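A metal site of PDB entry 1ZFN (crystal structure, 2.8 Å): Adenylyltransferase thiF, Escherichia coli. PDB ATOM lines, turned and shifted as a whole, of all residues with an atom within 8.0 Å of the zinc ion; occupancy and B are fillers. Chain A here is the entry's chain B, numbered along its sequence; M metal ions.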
ATOM      1  N   GLN A 135      18.505   9.067  -0.087  1.00  0.00           N
ATOM      2  CA  GLN A 135      18.381   9.752   1.182  1.00  0.00           C
ATOM      3  C   GLN A 135      19.528  10.741   1.388  1.00  0.00           C
ATOM      4  O   GLN A 135      19.338  11.796   1.991  1.00  0.00           O
ATOM      5  CB  GLN A 135      18.342   8.744   2.325  1.00  0.00           C
ATOM      6  CG  GLN A 135      17.030   7.980   2.401  1.00  0.00           C
ATOM      7  CD  GLN A 135      15.863   8.877   2.792  1.00  0.00           C
ATOM      8  OE1 GLN A 135      16.017  10.090   2.907  1.00  0.00           O
ATOM      9  NE2 GLN A 135      14.702   8.272   2.995  1.00  0.00           N
ATOM     10  N   ASN A 138      18.956  13.589  -1.304  1.00  0.00           N
ATOM     11  CA  ASN A 138      17.857  14.414  -0.829  1.00  0.00           C
ATOM     12  C   ASN A 138      18.318  15.460   0.175  1.00  0.00           C
ATOM     13  O   ASN A 138      17.937  16.631   0.086  1.00  0.00           O
ATOM     14  CB  ASN A 138      16.800  13.542  -0.159  1.00  0.00           C
ATOM     15  CG  ASN A 138      15.601  14.342   0.330  1.00  0.00           C
ATOM     16  OD1 ASN A 138      14.738  14.724  -0.456  1.00  0.00           O
ATOM     17  ND2 ASN A 138      15.558  14.606   1.615  1.00  0.00           N
ATOM     18  N   VAL A 142      18.037  19.463  -0.251  1.00  0.00           N
ATOM     19  CA  VAL A 142      17.251  20.319   0.633  1.00  0.00           C
ATOM     20  C   VAL A 142      18.149  21.343   1.297  1.00  0.00           C
ATOM     21  O   VAL A 142      17.767  22.501   1.459  1.00  0.00           O
ATOM     22  CB  VAL A 142      16.544  19.504   1.740  1.00  0.00           C
ATOM     23  CG1 VAL A 142      15.835  20.451   2.696  1.00  0.00           C
ATOM     24  CG2 VAL A 142      15.563  18.529   1.119  1.00  0.00           C
ATOM     25  N   LEU A 163      10.819  17.292  -6.358  1.00  0.00           N
ATOM     26  CA  LEU A 163      10.827  18.023  -5.091  1.00  0.00           C
ATOM     27  C   LEU A 163      11.571  19.333  -5.301  1.00  0.00           C
ATOM     28  O   LEU A 163      12.752  19.337  -5.661  1.00  0.00           O
ATOM     29  CB  LEU A 163      11.550  17.183  -4.039  1.00  0.00           C
ATOM     30  CG  LEU A 163      11.234  15.684  -4.082  1.00  0.00           C
ATOM     31  CD1 LEU A 163      11.990  14.978  -2.978  1.00  0.00           C
ATOM     32  CD2 LEU A 163       9.737  15.470  -3.923  1.00  0.00           C
ATOM     33  N   TRP A 167       9.877  23.485  -0.849  1.00  0.00           N
ATOM     34  CA  TRP A 167       9.684  22.238  -0.081  1.00  0.00           C
ATOM     35  C   TRP A 167       8.340  22.138   0.625  1.00  0.00           C
ATOM     36  O   TRP A 167       8.196  21.482   1.660  1.00  0.00           O
ATOM     37  CB  TRP A 167      10.808  22.073   0.950  1.00  0.00           C
ATOM     38  CG  TRP A 167      12.176  22.183   0.377  1.00  0.00           C
ATOM     39  CD1 TRP A 167      13.118  23.114   0.681  1.00  0.00           C
ATOM     40  CD2 TRP A 167      12.764  21.325  -0.614  1.00  0.00           C
ATOM     41  NE1 TRP A 167      14.254  22.903  -0.057  1.00  0.00           N
ATOM     42  CE2 TRP A 167      14.064  21.809  -0.852  1.00  0.00           C
ATOM     43  CE3 TRP A 167      12.317  20.199  -1.320  1.00  0.00           C
ATOM     44  CZ2 TRP A 167      14.937  21.205  -1.782  1.00  0.00           C
ATOM     45  CZ3 TRP A 167      13.181  19.601  -2.230  1.00  0.00           C
ATOM     46  CH2 TRP A 167      14.472  20.107  -2.449  1.00  0.00           C
ATOM     47  N   GLN A 169       5.675  20.432   0.130  1.00  0.00           N
ATOM     48  CA  GLN A 169       5.098  19.116   0.406  1.00  0.00           C
ATOM     49  C   GLN A 169       6.172  18.165   0.918  1.00  0.00           C
ATOM     50  O   GLN A 169       6.113  16.965   0.677  1.00  0.00           O
ATOM     51  CB  GLN A 169       4.446  18.510  -0.840  1.00  0.00           C
ATOM     52  CG  GLN A 169       4.576  19.313  -2.118  1.00  0.00           C
ATOM     53  CD  GLN A 169       3.567  20.447  -2.217  1.00  0.00           C
ATOM     54  OE1 GLN A 169       2.388  20.282  -1.885  1.00  0.00           O
ATOM     55  NE2 GLN A 169       4.015  21.601  -2.680  1.00  0.00           N
ATOM     56  N   GLY A 170       7.165  18.725   1.601  1.00  0.00           N
ATOM     57  CA  GLY A 170       8.231  17.923   2.146  1.00  0.00           C
ATOM     58  C   GLY A 170       9.229  17.391   1.146  1.00  0.00           C
ATOM     59  O   GLY A 170       9.133  17.680  -0.051  1.00  0.00           O
ATOM     60  N   CYS A 171      10.176  16.610   1.639  1.00  0.00           N
ATOM     61  CA  CYS A 171      11.212  16.003   0.819  1.00  0.00           C
ATOM     62  C   CYS A 171      11.099  14.488   0.905  1.00  0.00           C
ATOM     63  O   CYS A 171      10.084  13.977   1.380  1.00  0.00           O
ATOM     64  CB  CYS A 171      12.590  16.433   1.306  1.00  0.00           C
ATOM     65  SG  CYS A 171      13.017  15.752   2.901  1.00  0.00           S
ATOM     66  N   TYR A 172      12.145  13.785   0.462  1.00  0.00           N
ATOM     67  CA  TYR A 172      12.149  12.337   0.476  1.00  0.00           C
ATOM     68  C   TYR A 172      12.158  11.797   1.903  1.00  0.00           C
ATOM     69  O   TYR A 172      11.624  10.728   2.164  1.00  0.00           O
ATOM     70  CB  TYR A 172      13.373  11.804  -0.269  1.00  0.00           C
ATOM     71  CG  TYR A 172      13.263  10.369  -0.719  1.00  0.00           C
ATOM     72  CD1 TYR A 172      12.360   9.999  -1.708  1.00  0.00           C
ATOM     73  CD2 TYR A 172      14.092   9.389  -0.195  1.00  0.00           C
ATOM     74  CE1 TYR A 172      12.295   8.696  -2.177  1.00  0.00           C
ATOM     75  CE2 TYR A 172      14.036   8.067  -0.655  1.00  0.00           C
ATOM     76  CZ  TYR A 172      13.141   7.727  -1.648  1.00  0.00           C
ATOM     77  OH  TYR A 172      13.108   6.440  -2.136  1.00  0.00           O
ATOM     78  N   ARG A 173      12.775  12.533   2.817  1.00  0.00           N
ATOM     79  CA  ARG A 173      12.808  12.092   4.203  1.00  0.00           C
ATOM     80  C   ARG A 173      11.427  12.131   4.822  1.00  0.00           C
ATOM     81  O   ARG A 173      11.131  11.357   5.724  1.00  0.00           O
ATOM     82  CB  ARG A 173      13.757  12.955   5.025  1.00  0.00           C
ATOM     83  CG  ARG A 173      15.188  12.517   4.882  1.00  0.00           C
ATOM     84  CD  ARG A 173      16.099  13.369   5.728  1.00  0.00           C
ATOM     85  NE  ARG A 173      17.492  12.957   5.574  1.00  0.00           N
ATOM     86  CZ  ARG A 173      18.122  12.888   4.411  1.00  0.00           C
ATOM     87  NH1 ARG A 173      17.498  13.212   3.282  1.00  0.00           N
ATOM     88  NH2 ARG A 173      19.389  12.500   4.366  1.00  0.00           N
ATOM     89  N   CYS A 174      10.587  13.035   4.329  1.00  0.00           N
ATOM     90  CA  CYS A 174       9.226  13.119   4.837  1.00  0.00           C
ATOM     91  C   CYS A 174       8.420  11.900   4.387  1.00  0.00           C
ATOM     92  O   CYS A 174       7.510  11.458   5.081  1.00  0.00           O
ATOM     93  CB  CYS A 174       8.543  14.401   4.363  1.00  0.00           C
ATOM     94  SG  CYS A 174       9.229  15.926   5.061  1.00  0.00           S
ATOM     95  N   LEU A 175       8.753  11.360   3.211  1.00  0.00           N
ATOM     96  CA  LEU A 175       8.050  10.191   2.690  1.00  0.00           C
ATOM     97  C   LEU A 175       8.581   8.934   3.385  1.00  0.00           C
ATOM     98  O   LEU A 175       7.805   8.120   3.878  1.00  0.00           O
ATOM     99  CB  LEU A 175       8.242  10.083   1.175  1.00  0.00           C
ATOM    100  CG  LEU A 175       7.690   8.848   0.440  1.00  0.00           C
ATOM    101  CD1 LEU A 175       6.209   8.678   0.724  1.00  0.00           C
ATOM    102  CD2 LEU A 175       7.937   8.973  -1.064  1.00  0.00           C
ATOM    103  N   TRP A 176       9.906   8.789   3.398  1.00  0.00           N
ATOM    104  CA  TRP A 176      10.580   7.645   4.001  1.00  0.00           C
ATOM    105  C   TRP A 176      11.506   8.075   5.140  1.00  0.00           C
ATOM    106  O   TRP A 176      11.121   8.044   6.316  1.00  0.00           O
ATOM    107  CB  TRP A 176      11.380   6.879   2.938  1.00  0.00           C
ATOM    108  CG  TRP A 176      10.620   5.733   2.357  1.00  0.00           C
ATOM    109  CD1 TRP A 176      10.264   4.577   2.996  1.00  0.00           C
ATOM    110  CD2 TRP A 176      10.079   5.630   1.030  1.00  0.00           C
ATOM    111  NE1 TRP A 176       9.532   3.768   2.161  1.00  0.00           N
ATOM    112  CE2 TRP A 176       9.400   4.390   0.944  1.00  0.00           C
ATOM    113  CE3 TRP A 176      10.092   6.459  -0.098  1.00  0.00           C
ATOM    114  CZ2 TRP A 176       8.750   3.954  -0.229  1.00  0.00           C
ATOM    115  CZ3 TRP A 176       9.450   6.028  -1.268  1.00  0.00           C
ATOM    116  CH2 TRP A 176       8.781   4.792  -1.314  1.00  0.00           C
ATOM    117  N   ARG A 237       3.168  14.937   1.609  1.00  0.00           N
ATOM    118  CA  ARG A 237       2.971  15.922   2.666  1.00  0.00           C
ATOM    119  C   ARG A 237       4.227  15.974   3.508  1.00  0.00           C
ATOM    120  O   ARG A 237       4.782  14.930   3.863  1.00  0.00           O
ATOM    121  CB  ARG A 237       1.751  15.552   3.519  1.00  0.00           C
ATOM    122  CG  ARG A 237       1.830  14.208   4.219  1.00  0.00           C
ATOM    123  CD  ARG A 237       2.425  14.322   5.622  1.00  0.00           C
ATOM    124  NE  ARG A 237       1.639  15.178   6.507  1.00  0.00           N
ATOM    125  CZ  ARG A 237       1.849  15.312   7.806  1.00  0.00           C
ATOM    126  NH1 ARG A 237       2.845  14.650   8.401  1.00  0.00           N
ATOM    127  NH2 ARG A 237       1.075  16.112   8.538  1.00  0.00           N
ATOM    128  N   ARG A 238       4.696  17.185   3.795  1.00  0.00           N
ATOM    129  CA  ARG A 238       5.897  17.322   4.601  1.00  0.00           C
ATOM    130  C   ARG A 238       5.600  16.840   6.017  1.00  0.00           C
ATOM    131  O   ARG A 238       4.514  17.076   6.556  1.00  0.00           O
ATOM    132  CB  ARG A 238       6.373  18.773   4.625  1.00  0.00           C
ATOM    133  CG  ARG A 238       5.358  19.743   5.124  1.00  0.00           C
ATOM    134  CD  ARG A 238       5.974  21.106   5.232  1.00  0.00           C
ATOM    135  NE  ARG A 238       5.002  22.081   5.701  1.00  0.00           N
ATOM    136  CZ  ARG A 238       5.294  23.350   5.928  1.00  0.00           C
ATOM    137  NH1 ARG A 238       6.529  23.801   5.726  1.00  0.00           N
ATOM    138  NH2 ARG A 238       4.343  24.182   6.353  1.00  0.00           N
ATOM    139  N   ALA A 239       6.574  16.155   6.611  1.00  0.00           N
ATOM    140  CA  ALA A 239       6.425  15.617   7.952  1.00  0.00           C
ATOM    141  C   ALA A 239       6.564  16.681   9.034  1.00  0.00           C
ATOM    142  O   ALA A 239       7.566  17.408   9.068  1.00  0.00           O
ATOM    143  CB  ALA A 239       7.435  14.510   8.179  1.00  0.00           C
ATOM    144  N   SER A 240       5.563  16.761   9.913  1.00  0.00           N
ATOM    145  CA  SER A 240       5.580  17.714  11.020  1.00  0.00           C
ATOM    146  C   SER A 240       6.881  17.439  11.768  1.00  0.00           C
ATOM    147  O   SER A 240       7.039  16.375  12.355  1.00  0.00           O
ATOM    148  CB  SER A 240       4.388  17.455  11.945  1.00  0.00           C
ATOM    149  OG  SER A 240       3.180  17.342  11.227  1.00  0.00           O
ATOM    150  N   GLY A 241       7.799  18.406  11.740  1.00  0.00           N
ATOM    151  CA  GLY A 241       9.071  18.194  12.414  1.00  0.00           C
ATOM    152  C   GLY A 241       9.816  17.094  11.678  1.00  0.00           C
ATOM    153  O   GLY A 241       9.571  15.909  11.891  1.00  0.00           O
ATOM    154  N   CYS A 242      10.728  17.493  10.805  1.00  0.00           N
ATOM    155  CA  CYS A 242      11.502  16.552  10.009  1.00  0.00           C
ATOM    156  C   CYS A 242      12.995  16.894  10.062  1.00  0.00           C
ATOM    157  O   CYS A 242      13.361  18.057  10.159  1.00  0.00           O
ATOM    158  CB  CYS A 242      10.997  16.609   8.559  1.00  0.00           C
ATOM    159  SG  CYS A 242      12.091  15.864   7.351  1.00  0.00           S
ATOM    160  N   PRO A 243      13.862  15.868  10.003  1.00  0.00           N
ATOM    161  CA  PRO A 243      15.316  16.004  10.051  1.00  0.00           C
ATOM    162  C   PRO A 243      15.918  16.910   8.974  1.00  0.00           C
ATOM    163  O   PRO A 243      17.115  17.177   8.984  1.00  0.00           O
ATOM    164  CB  PRO A 243      15.807  14.574   9.905  1.00  0.00           C
ATOM    165  CG  PRO A 243      14.757  13.799  10.588  1.00  0.00           C
ATOM    166  CD  PRO A 243      13.476  14.454  10.083  1.00  0.00           C
ATOM    167  N   VAL A 244      15.090  17.373   8.039  1.00  0.00           N
ATOM    168  CA  VAL A 244      15.585  18.244   6.981  1.00  0.00           C
ATOM    169  C   VAL A 244      14.695  19.461   6.847  1.00  0.00           C
ATOM    170  O   VAL A 244      14.950  20.492   7.460  1.00  0.00           O
ATOM    171  CB  VAL A 244      15.661  17.501   5.636  1.00  0.00           C
ATOM    172  CG1 VAL A 244      16.887  16.617   5.597  1.00  0.00           C
ATOM    173  CG2 VAL A 244      14.423  16.660   5.451  1.00  0.00           C
ATOM    174  N   CYS A 245      13.636  19.350   6.048  1.00  0.00           N
ATOM    175  CA  CYS A 245      12.734  20.493   5.908  1.00  0.00           C
ATOM    176  C   CYS A 245      12.219  20.944   7.284  1.00  0.00           C
ATOM    177  O   CYS A 245      11.274  20.368   7.822  1.00  0.00           O
ATOM    178  CB  CYS A 245      11.570  20.134   4.979  1.00  0.00           C
ATOM    179  SG  CYS A 245      10.982  18.449   5.112  1.00  0.00           S
ATOM    180  N   GLY A 246      12.872  21.967   7.865  1.00  0.00           N
ATOM    181  CA  GLY A 246      12.492  22.490   9.181  1.00  0.00           C
ATOM    182  C   GLY A 246      12.199  23.995   9.258  1.00  0.00           C
ATOM    183  O   GLY A 246      12.112  24.725   8.251  1.00  0.00           O
HETATM  184 ZN    ZN M   1      11.540  16.147   4.747  1.00  0.00          ZN
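The zinc ion is bound by SG of Cys 174 (2.3 Å). The zinc ion is bound by SG of Cys 245 (2.4 Å). The zinc ion is bound by SG of Cys 171. The zinc ion is bound by the side-chain sulfur (SG) of Cys 242.
Arg 173 touches the zinc ion (CB to ZN, 3.9 Å). Val 244 touches the zinc ion (CG2 to ZN, 3.0 Å). Six residues have an atom within 4 Å of the zinc ion: Cys 171, Arg 173, Cys 174, Cys 242, Val 244 and Cys 245.
SG of Cys 171 sits close to ND2 of Asn 138 (3.1 Å). The side-chain sulfur (SG) of Cys 174 lies close to the backbone NH (N) of Ala 239 (3.1 Å). N of Arg 173 sits close to SG of Cys 171, 3.2 Å away. NH1 of Arg 173 lies close to ND2 of Asn 138, at 2.9 Å. SG of Cys 242 sits close to N of Val 244 (3.4 Å). The guanidinium group (NH2) of Arg 173 sits at hydrogen-bond distance from the backbone carbonyl oxygen (O) of Gln 135, 2.5 Å away.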
